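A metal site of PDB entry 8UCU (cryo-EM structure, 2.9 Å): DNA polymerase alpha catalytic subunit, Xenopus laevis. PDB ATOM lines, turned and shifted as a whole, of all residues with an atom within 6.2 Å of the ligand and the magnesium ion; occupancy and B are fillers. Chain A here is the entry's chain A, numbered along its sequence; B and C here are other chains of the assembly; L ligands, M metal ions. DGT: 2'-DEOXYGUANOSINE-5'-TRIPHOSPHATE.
A nitrogen (N2) of the ligand sits close to N9 of DG 17 of chain B (3.4 Å).
The guanidinium group (NH2) of Arg 587 lies within salt-bridge range of an oxygen (O2G) of the ligand (2.6 Å).
N of Ser 531 is in hydrogen-bond range of O3B of the ligand.
O3G of the ligand is in hydrogen-bond range of ND2 of Asn 530 (3.3 Å).
An oxygen (O1B) of the ligand lies within hydrogen-bond range of the backbone NH (N) of Leu 532.
The backbone NH of Tyr 533 is in hydrogen-bond range of an oxygen (O3') of the ligand (2.9 Å).
O2 of DC 16 of chain B sits at hydrogen-bond distance from a nitrogen (N2) of the ligand (2.7 Å).
NZ of Lys 615 lies within salt-bridge range of O2A of the ligand (3.2 Å).
A nitrogen (N2) of the ligand sits at hydrogen-bond distance from the backbone carbonyl oxygen (O) of Asn 619, 3.2 Å away.
NH2 of Arg 587 sits close to NE2 of Gln 611 (3.5 Å).
N2 of DG 17 of chain B sits close to O2 of DOC 29 of chain C, 2.7 Å away.
The side-chain hydroxyl of Ser 620 sits at hydrogen-bond distance from the backbone carbonyl oxygen of Leu 616.
The side-chain amide nitrogen of Asn 619 lies close to the backbone carbonyl oxygen of Lys 615, 3.4 Å away.
N3 of DOC 29 of chain C lies close to N7 of the ligand, 3.2 Å away.
Merely in contact with the ligand: Leu 616 (3.3 Å), Tyr 622 (3.3 Å) and Gly 623 (3.9 Å).
Hydrophobic or aromatic side chains that line the ligand: Leu 532, Tyr 533, Leu 616 and Tyr 622.
Of the 23 residues printed, 16 come within 4 Å of the ligand.
Within 4 Å of the magnesium ion: Asp 528, Phe 529 and Asp 669.
The nearest printed residue that does not touch the magnesium ion is Asn 530 (4.5 Å).
The magnesium ion is bound by OD2 of Asp 528 (1.9 Å), OD2 of Asp 669 (2.1 Å), O1G of the ligand (2.1 Å), O2B of the ligand (2.2 Å), O1A of the ligand (2.2 Å) and O of Phe 529 (2.3 Å).
The magnesium ion has six donor atoms within binding distance.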
ATOM      1  N   ASP A 528      29.745 -33.069  23.466  1.00  0.00           N
ATOM      2  CA  ASP A 528      28.991 -31.845  23.691  1.00  0.00           C
ATOM      3  C   ASP A 528      27.798 -32.132  24.595  1.00  0.00           C
ATOM      4  O   ASP A 528      27.112 -33.144  24.415  1.00  0.00           O
ATOM      5  CB  ASP A 528      28.506 -31.242  22.377  1.00  0.00           C
ATOM      6  CG  ASP A 528      27.980 -29.823  22.530  1.00  0.00           C
ATOM      7  OD1 ASP A 528      28.780 -28.880  22.428  1.00  0.00           O
ATOM      8  OD2 ASP A 528      26.761 -29.661  22.762  1.00  0.00           O
ATOM      9  N   PHE A 529      27.554 -31.244  25.546  1.00  0.00           N
ATOM     10  CA  PHE A 529      26.408 -31.385  26.425  1.00  0.00           C
ATOM     11  C   PHE A 529      25.117 -31.054  25.674  1.00  0.00           C
ATOM     12  O   PHE A 529      25.099 -30.252  24.734  1.00  0.00           O
ATOM     13  CB  PHE A 529      26.541 -30.474  27.640  1.00  0.00           C
ATOM     14  CG  PHE A 529      27.253 -31.109  28.796  1.00  0.00           C
ATOM     15  CD1 PHE A 529      26.600 -32.014  29.614  1.00  0.00           C
ATOM     16  CD2 PHE A 529      28.576 -30.814  29.066  1.00  0.00           C
ATOM     17  CE1 PHE A 529      27.246 -32.602  30.674  1.00  0.00           C
ATOM     18  CE2 PHE A 529      29.231 -31.398  30.124  1.00  0.00           C
ATOM     19  CZ  PHE A 529      28.561 -32.289  30.934  1.00  0.00           C
ATOM     20  N   ASN A 530      24.027 -31.675  26.114  1.00  0.00           N
ATOM     21  CA  ASN A 530      22.702 -31.461  25.557  1.00  0.00           C
ATOM     22  C   ASN A 530      21.971 -30.421  26.397  1.00  0.00           C
ATOM     23  O   ASN A 530      21.750 -30.647  27.591  1.00  0.00           O
ATOM     24  CB  ASN A 530      21.913 -32.767  25.520  1.00  0.00           C
ATOM     25  CG  ASN A 530      22.301 -33.657  24.360  1.00  0.00           C
ATOM     26  OD1 ASN A 530      22.718 -34.801  24.556  1.00  0.00           O
ATOM     27  ND2 ASN A 530      22.150 -33.148  23.153  1.00  0.00           N
ATOM     28  N   SER A 531      21.589 -29.315  25.775  1.00  0.00           N
ATOM     29  CA  SER A 531      20.855 -28.247  26.451  1.00  0.00           C
ATOM     30  C   SER A 531      21.493 -27.941  27.806  1.00  0.00           C
ATOM     31  O   SER A 531      20.894 -28.112  28.861  1.00  0.00           O
ATOM     32  CB  SER A 531      19.384 -28.613  26.598  1.00  0.00           C
ATOM     33  OG  SER A 531      19.238 -29.839  27.293  1.00  0.00           O
ATOM     34  N   LEU A 532      22.739 -27.467  27.740  1.00  0.00           N
ATOM     35  CA  LEU A 532      23.559 -27.383  28.946  1.00  0.00           C
ATOM     36  C   LEU A 532      22.944 -26.456  29.980  1.00  0.00           C
ATOM     37  O   LEU A 532      22.889 -26.777  31.170  1.00  0.00           O
ATOM     38  CB  LEU A 532      24.975 -26.923  28.598  1.00  0.00           C
ATOM     39  CG  LEU A 532      25.899 -26.745  29.804  1.00  0.00           C
ATOM     40  CD1 LEU A 532      26.033 -28.053  30.572  1.00  0.00           C
ATOM     41  CD2 LEU A 532      27.264 -26.242  29.379  1.00  0.00           C
ATOM     42  N   TYR A 533      22.481 -25.280  29.566  1.00  0.00           N
ATOM     43  CA  TYR A 533      21.988 -24.306  30.531  1.00  0.00           C
ATOM     44  C   TYR A 533      20.586 -24.673  30.993  1.00  0.00           C
ATOM     45  O   TYR A 533      20.274 -24.579  32.187  1.00  0.00           O
ATOM     46  CB  TYR A 533      22.011 -22.891  29.929  1.00  0.00           C
ATOM     47  CG  TYR A 533      23.381 -22.249  29.969  1.00  0.00           C
ATOM     48  CD1 TYR A 533      24.539 -23.001  29.895  1.00  0.00           C
ATOM     49  CD2 TYR A 533      23.511 -20.865  30.072  1.00  0.00           C
ATOM     50  CE1 TYR A 533      25.780 -22.420  29.924  1.00  0.00           C
ATOM     51  CE2 TYR A 533      24.750 -20.274  30.111  1.00  0.00           C
ATOM     52  CZ  TYR A 533      25.885 -21.057  30.033  1.00  0.00           C
ATOM     53  OH  TYR A 533      27.124 -20.466  30.071  1.00  0.00           O
ATOM     54  N   PRO A 534      19.697 -25.079  30.080  1.00  0.00           N
ATOM     55  CA  PRO A 534      18.425 -25.674  30.530  1.00  0.00           C
ATOM     56  C   PRO A 534      18.640 -26.840  31.480  1.00  0.00           C
ATOM     57  O   PRO A 534      17.942 -26.964  32.494  1.00  0.00           O
ATOM     58  CB  PRO A 534      17.783 -26.120  29.216  1.00  0.00           C
ATOM     59  CG  PRO A 534      18.290 -25.157  28.220  1.00  0.00           C
ATOM     60  CD  PRO A 534      19.683 -24.821  28.630  1.00  0.00           C
ATOM     61  N   ARG A 587      11.734 -30.137  22.409  1.00  0.00           N
ATOM     62  CA  ARG A 587      12.848 -30.193  21.466  1.00  0.00           C
ATOM     63  C   ARG A 587      13.352 -31.620  21.286  1.00  0.00           C
ATOM     64  O   ARG A 587      13.672 -32.042  20.164  1.00  0.00           O
ATOM     65  CB  ARG A 587      13.988 -29.289  21.941  1.00  0.00           C
ATOM     66  CG  ARG A 587      14.959 -28.919  20.856  1.00  0.00           C
ATOM     67  CD  ARG A 587      16.258 -28.392  21.417  1.00  0.00           C
ATOM     68  NE  ARG A 587      17.390 -28.739  20.562  1.00  0.00           N
ATOM     69  CZ  ARG A 587      18.654 -28.722  20.949  1.00  0.00           C
ATOM     70  NH1 ARG A 587      19.001 -28.360  22.175  1.00  0.00           N
ATOM     71  NH2 ARG A 587      19.599 -29.067  20.077  1.00  0.00           N
ATOM     72  N   LYS A 591      13.596 -33.831  17.859  1.00  0.00           N
ATOM     73  CA  LYS A 591      14.851 -34.445  17.420  1.00  0.00           C
ATOM     74  C   LYS A 591      14.682 -35.942  17.198  1.00  0.00           C
ATOM     75  O   LYS A 591      15.168 -36.490  16.205  1.00  0.00           O
ATOM     76  CB  LYS A 591      15.955 -34.168  18.426  1.00  0.00           C
ATOM     77  CG  LYS A 591      16.654 -32.836  18.220  1.00  0.00           C
ATOM     78  CD  LYS A 591      17.739 -32.609  19.252  1.00  0.00           C
ATOM     79  CE  LYS A 591      19.110 -32.516  18.601  1.00  0.00           C
ATOM     80  NZ  LYS A 591      20.201 -32.319  19.593  1.00  0.00           N
ATOM     81  N   GLN A 611      13.557 -27.565  15.577  1.00  0.00           N
ATOM     82  CA  GLN A 611      14.415 -27.919  16.706  1.00  0.00           C
ATOM     83  C   GLN A 611      15.320 -26.754  17.082  1.00  0.00           C
ATOM     84  O   GLN A 611      15.506 -26.466  18.271  1.00  0.00           O
ATOM     85  CB  GLN A 611      15.242 -29.159  16.343  1.00  0.00           C
ATOM     86  CG  GLN A 611      16.585 -29.310  17.044  1.00  0.00           C
ATOM     87  CD  GLN A 611      17.751 -29.011  16.132  1.00  0.00           C
ATOM     88  OE1 GLN A 611      17.662 -29.144  14.910  1.00  0.00           O
ATOM     89  NE2 GLN A 611      18.878 -28.615  16.723  1.00  0.00           N
ATOM     90  N   LYS A 615      15.432 -24.788  20.663  1.00  0.00           N
ATOM     91  CA  LYS A 615      16.698 -24.571  21.360  1.00  0.00           C
ATOM     92  C   LYS A 615      16.888 -23.096  21.672  1.00  0.00           C
ATOM     93  O   LYS A 615      17.260 -22.727  22.793  1.00  0.00           O
ATOM     94  CB  LYS A 615      17.855 -25.091  20.514  1.00  0.00           C
ATOM     95  CG  LYS A 615      19.222 -24.880  21.148  1.00  0.00           C
ATOM     96  CD  LYS A 615      20.294 -25.709  20.454  1.00  0.00           C
ATOM     97  CE  LYS A 615      21.065 -24.911  19.426  1.00  0.00           C
ATOM     98  NZ  LYS A 615      22.506 -24.816  19.746  1.00  0.00           N
ATOM     99  N   LEU A 616      16.636 -22.235  20.697  1.00  0.00           N
ATOM    100  CA  LEU A 616      16.797 -20.805  20.915  1.00  0.00           C
ATOM    101  C   LEU A 616      15.785 -20.269  21.904  1.00  0.00           C
ATOM    102  O   LEU A 616      16.082 -19.346  22.654  1.00  0.00           O
ATOM    103  CB  LEU A 616      16.694 -20.043  19.594  1.00  0.00           C
ATOM    104  CG  LEU A 616      18.000 -19.556  18.945  1.00  0.00           C
ATOM    105  CD1 LEU A 616      17.684 -18.671  17.754  1.00  0.00           C
ATOM    106  CD2 LEU A 616      18.874 -18.800  19.937  1.00  0.00           C
ATOM    107  N   ASN A 619      17.231 -21.190  25.269  1.00  0.00           N
ATOM    108  CA  ASN A 619      18.406 -20.373  25.534  1.00  0.00           C
ATOM    109  C   ASN A 619      18.028 -18.927  25.807  1.00  0.00           C
ATOM    110  O   ASN A 619      18.657 -18.269  26.645  1.00  0.00           O
ATOM    111  CB  ASN A 619      19.382 -20.465  24.368  1.00  0.00           C
ATOM    112  CG  ASN A 619      20.110 -21.802  24.326  1.00  0.00           C
ATOM    113  OD1 ASN A 619      20.212 -22.485  25.339  1.00  0.00           O
ATOM    114  ND2 ASN A 619      20.615 -22.163  23.157  1.00  0.00           N
ATOM    115  N   SER A 620      17.009 -18.402  25.131  1.00  0.00           N
ATOM    116  CA  SER A 620      16.521 -17.063  25.406  1.00  0.00           C
ATOM    117  C   SER A 620      15.831 -16.996  26.759  1.00  0.00           C
ATOM    118  O   SER A 620      15.889 -15.963  27.431  1.00  0.00           O
ATOM    119  CB  SER A 620      15.580 -16.602  24.300  1.00  0.00           C
ATOM    120  OG  SER A 620      16.146 -16.823  23.023  1.00  0.00           O
ATOM    121  N   TYR A 622      16.889 -18.610  29.281  1.00  0.00           N
ATOM    122  CA  TYR A 622      18.054 -18.387  30.121  1.00  0.00           C
ATOM    123  C   TYR A 622      18.521 -16.940  30.037  1.00  0.00           C
ATOM    124  O   TYR A 622      18.773 -16.297  31.064  1.00  0.00           O
ATOM    125  CB  TYR A 622      19.197 -19.312  29.717  1.00  0.00           C
ATOM    126  CG  TYR A 622      20.551 -18.642  29.868  1.00  0.00           C
ATOM    127  CD1 TYR A 622      21.059 -18.346  31.128  1.00  0.00           C
ATOM    128  CD2 TYR A 622      21.301 -18.294  28.762  1.00  0.00           C
ATOM    129  CE1 TYR A 622      22.281 -17.727  31.268  1.00  0.00           C
ATOM    130  CE2 TYR A 622      22.522 -17.676  28.892  1.00  0.00           C
ATOM    131  CZ  TYR A 622      23.010 -17.388  30.145  1.00  0.00           C
ATOM    132  OH  TYR A 622      24.226 -16.783  30.287  1.00  0.00           O
ATOM    133  N   GLY A 623      18.665 -16.412  28.822  1.00  0.00           N
ATOM    134  CA  GLY A 623      19.309 -15.123  28.646  1.00  0.00           C
ATOM    135  C   GLY A 623      18.508 -13.975  29.225  1.00  0.00           C
ATOM    136  O   GLY A 623      19.076 -13.025  29.767  1.00  0.00           O
ATOM    137  N   CYS A 624      17.178 -14.045  29.132  1.00  0.00           N
ATOM    138  CA  CYS A 624      16.342 -12.955  29.618  1.00  0.00           C
ATOM    139  C   CYS A 624      16.469 -12.760  31.114  1.00  0.00           C
ATOM    140  O   CYS A 624      16.076 -11.713  31.628  1.00  0.00           O
ATOM    141  CB  CYS A 624      14.887 -13.208  29.230  1.00  0.00           C
ATOM    142  SG  CYS A 624      14.548 -12.986  27.470  1.00  0.00           S
ATOM    143  N   ASP A 667      34.467 -25.297  24.331  1.00  0.00           N
ATOM    144  CA  ASP A 667      33.780 -23.998  24.330  1.00  0.00           C
ATOM    145  C   ASP A 667      32.488 -24.101  25.123  1.00  0.00           C
ATOM    146  O   ASP A 667      31.405 -24.286  24.573  1.00  0.00           O
ATOM    147  CB  ASP A 667      33.529 -23.542  22.896  1.00  0.00           C
ATOM    148  CG  ASP A 667      32.963 -22.132  22.832  1.00  0.00           C
ATOM    149  OD1 ASP A 667      32.852 -21.490  23.894  1.00  0.00           O
ATOM    150  OD2 ASP A 667      32.632 -21.680  21.722  1.00  0.00           O
ATOM    151  N   THR A 668      32.619 -23.983  26.442  1.00  0.00           N
ATOM    152  CA  THR A 668      31.512 -23.732  27.361  1.00  0.00           C
ATOM    153  C   THR A 668      30.586 -24.926  27.565  1.00  0.00           C
ATOM    154  O   THR A 668      29.816 -24.940  28.531  1.00  0.00           O
ATOM    155  CB  THR A 668      30.683 -22.540  26.859  1.00  0.00           C
ATOM    156  OG1 THR A 668      31.536 -21.417  26.638  1.00  0.00           O
ATOM    157  CG2 THR A 668      29.597 -22.172  27.858  1.00  0.00           C
ATOM    158  N   ASP A 669      30.645 -25.918  26.695  1.00  0.00           N
ATOM    159  CA  ASP A 669      29.949 -27.171  26.976  1.00  0.00           C
ATOM    160  C   ASP A 669      30.611 -28.395  26.360  1.00  0.00           C
ATOM    161  O   ASP A 669      30.045 -29.483  26.492  1.00  0.00           O
ATOM    162  CB  ASP A 669      28.487 -27.062  26.535  1.00  0.00           C
ATOM    163  CG  ASP A 669      28.287 -27.392  25.077  1.00  0.00           C
ATOM    164  OD1 ASP A 669      29.175 -27.093  24.260  1.00  0.00           O
ATOM    165  OD2 ASP A 669      27.205 -27.938  24.753  1.00  0.00           O
ATOM    166  P    DC B  16      14.818  -9.253  22.087  1.00  0.00           P
ATOM    167  OP1  DC B  16      15.317 -10.225  21.100  1.00  0.00           O
ATOM    168  OP2  DC B  16      13.367  -9.043  22.264  1.00  0.00           O
ATOM    169  O5'  DC B  16      15.455  -9.624  23.497  1.00  0.00           O
ATOM    170  C5'  DC B  16      16.856  -9.503  23.699  1.00  0.00           C
ATOM    171  C4'  DC B  16      17.335 -10.423  24.801  1.00  0.00           C
ATOM    172  O4'  DC B  16      16.956 -11.779  24.474  1.00  0.00           O
ATOM    173  C3'  DC B  16      18.836 -10.479  24.992  1.00  0.00           C
ATOM    174  O3'  DC B  16      19.282  -9.431  25.836  1.00  0.00           O
ATOM    175  C2'  DC B  16      19.036 -11.849  25.604  1.00  0.00           C
ATOM    176  C1'  DC B  16      17.948 -12.683  24.936  1.00  0.00           C
ATOM    177  N1   DC B  16      18.445 -13.466  23.775  1.00  0.00           N
ATOM    178  C2   DC B  16      19.316 -14.539  23.991  1.00  0.00           C
ATOM    179  O2   DC B  16      19.642 -14.820  25.151  1.00  0.00           O
ATOM    180  N3   DC B  16      19.765 -15.242  22.932  1.00  0.00           N
ATOM    181  C4   DC B  16      19.380 -14.921  21.706  1.00  0.00           C
ATOM    182  N4   DC B  16      19.854 -15.646  20.686  1.00  0.00           N
ATOM    183  C5   DC B  16      18.508 -13.827  21.459  1.00  0.00           C
ATOM    184  C6   DC B  16      18.062 -13.134  22.508  1.00  0.00           C
ATOM    185  P    DG B  17      20.820  -8.971  25.796  1.00  0.00           P
ATOM    186  OP1  DG B  17      20.967  -7.782  26.668  1.00  0.00           O
ATOM    187  OP2  DG B  17      21.234  -8.911  24.378  1.00  0.00           O
ATOM    188  O5'  DG B  17      21.601 -10.189  26.488  1.00  0.00           O
ATOM    189  C5'  DG B  17      21.363 -10.504  27.841  1.00  0.00           C
ATOM    190  C4'  DG B  17      22.253 -11.641  28.311  1.00  0.00           C
ATOM    191  O4'  DG B  17      21.903 -12.853  27.617  1.00  0.00           O
ATOM    192  C3'  DG B  17      23.731 -11.445  28.064  1.00  0.00           C
ATOM    193  O3'  DG B  17      24.333 -10.740  29.134  1.00  0.00           O
ATOM    194  C2'  DG B  17      24.244 -12.868  27.954  1.00  0.00           C
ATOM    195  C1'  DG B  17      23.060 -13.641  27.375  1.00  0.00           C
ATOM    196  N9   DG B  17      23.151 -13.899  25.946  1.00  0.00           N
ATOM    197  C8   DG B  17      22.514 -13.232  24.941  1.00  0.00           C
ATOM    198  N7   DG B  17      22.777 -13.699  23.758  1.00  0.00           N
ATOM    199  C5   DG B  17      23.652 -14.749  23.992  1.00  0.00           C
ATOM    200  C6   DG B  17      24.292 -15.632  23.092  1.00  0.00           C
ATOM    201  O6   DG B  17      24.193 -15.661  21.854  1.00  0.00           O
ATOM    202  N1   DG B  17      25.103 -16.549  23.750  1.00  0.00           N
ATOM    203  C2   DG B  17      25.275 -16.608  25.106  1.00  0.00           C
ATOM    204  N2   DG B  17      26.100 -17.555  25.561  1.00  0.00           N
ATOM    205  N3   DG B  17      24.683 -15.781  25.962  1.00  0.00           N
ATOM    206  C4   DG B  17      23.897 -14.886  25.344  1.00  0.00           C
ATOM    207  N1  DOC C  29      27.875 -20.256  21.976  1.00  0.00           N
ATOM    208  C2  DOC C  29      27.241 -19.299  22.678  1.00  0.00           C
ATOM    209  N3  DOC C  29      26.303 -18.548  22.118  1.00  0.00           N
ATOM    210  C4  DOC C  29      25.976 -18.699  20.846  1.00  0.00           C
ATOM    211  C5  DOC C  29      26.622 -19.684  20.084  1.00  0.00           C
ATOM    212  C6  DOC C  29      27.570 -20.453  20.664  1.00  0.00           C
ATOM    213  O2  DOC C  29      27.527 -19.134  23.853  1.00  0.00           O
ATOM    214  N4  DOC C  29      25.000 -17.908  20.278  1.00  0.00           N
ATOM    215  C1' DOC C  29      28.912 -21.064  22.618  1.00  0.00           C
ATOM    216  C2' DOC C  29      28.268 -22.125  23.526  1.00  0.00           C
ATOM    217  C3' DOC C  29      28.307 -23.382  22.636  1.00  0.00           C
ATOM    218  C4' DOC C  29      29.636 -23.168  21.871  1.00  0.00           C
ATOM    219  O4' DOC C  29      29.711 -21.747  21.635  1.00  0.00           O
ATOM    220  C5' DOC C  29      29.632 -23.945  20.560  1.00  0.00           C
ATOM    221  O5' DOC C  29      30.155 -23.126  19.521  1.00  0.00           O
ATOM    222  P   DOC C  29      29.971 -23.580  17.989  1.00  0.00           P
ATOM    223  OP1 DOC C  29      30.647 -24.877  17.779  1.00  0.00           O
ATOM    224  OP2 DOC C  29      28.431 -23.405  17.562  1.00  0.00           O
HETATM  225  PG  DGT L   1      22.489 -28.686  22.137  1.00  0.00           P
HETATM  226  O1G DGT L   1      24.091 -28.857  22.121  1.00  0.00           O
HETATM  227  O2G DGT L   1      21.975 -28.291  20.669  1.00  0.00           O
HETATM  228  O3G DGT L   1      21.866 -29.963  22.552  1.00  0.00           O
HETATM  229  O3B DGT L   1      22.124 -27.532  23.186  1.00  0.00           O
HETATM  230  PB  DGT L   1      23.058 -26.499  23.991  1.00  0.00           P
HETATM  231  O1B DGT L   1      22.186 -25.681  25.054  1.00  0.00           O
HETATM  232  O2B DGT L   1      24.141 -27.245  24.663  1.00  0.00           O
HETATM  233  O3A DGT L   1      23.701 -25.462  22.943  1.00  0.00           O
HETATM  234  PA  DGT L   1      25.220 -25.113  22.569  1.00  0.00           P
HETATM  235  O1A DGT L   1      26.056 -26.484  22.506  1.00  0.00           O
HETATM  236  O2A DGT L   1      25.263 -24.444  21.257  1.00  0.00           O
HETATM  237  O5' DGT L   1      25.791 -24.108  23.694  1.00  0.00           O
HETATM  238  C5' DGT L   1      25.810 -24.429  25.086  1.00  0.00           C
HETATM  239  C4' DGT L   1      25.342 -23.233  25.923  1.00  0.00           C
HETATM  240  O4' DGT L   1      25.681 -21.974  25.292  1.00  0.00           O
HETATM  241  C3' DGT L   1      23.795 -23.201  26.012  1.00  0.00           C
HETATM  242  O3' DGT L   1      23.326 -24.085  27.028  1.00  0.00           O
HETATM  243  C2' DGT L   1      23.579 -21.732  26.415  1.00  0.00           C
HETATM  244  C1' DGT L   1      24.646 -21.009  25.578  1.00  0.00           C
HETATM  245  N9  DGT L   1      24.051 -20.480  24.344  1.00  0.00           N
HETATM  246  C8  DGT L   1      24.236 -20.946  23.080  1.00  0.00           C
HETATM  247  N7  DGT L   1      23.553 -20.230  22.249  1.00  0.00           N
HETATM  248  C5  DGT L   1      22.890 -19.263  22.923  1.00  0.00           C
HETATM  249  C6  DGT L   1      22.007 -18.218  22.549  1.00  0.00           C
HETATM  250  O6  DGT L   1      21.710 -18.044  21.383  1.00  0.00           O
HETATM  251  N1  DGT L   1      21.520 -17.424  23.516  1.00  0.00           N
HETATM  252  C2  DGT L   1      21.870 -17.629  24.819  1.00  0.00           C
HETATM  253  N2  DGT L   1      21.349 -16.806  25.778  1.00  0.00           N
HETATM  254  N3  DGT L   1      22.678 -18.596  25.177  1.00  0.00           N
HETATM  255  C4  DGT L   1      23.205 -19.416  24.268  1.00  0.00           C
HETATM  256 MG    MG M   1      25.593 -28.364  23.517  1.00  0.00          MG
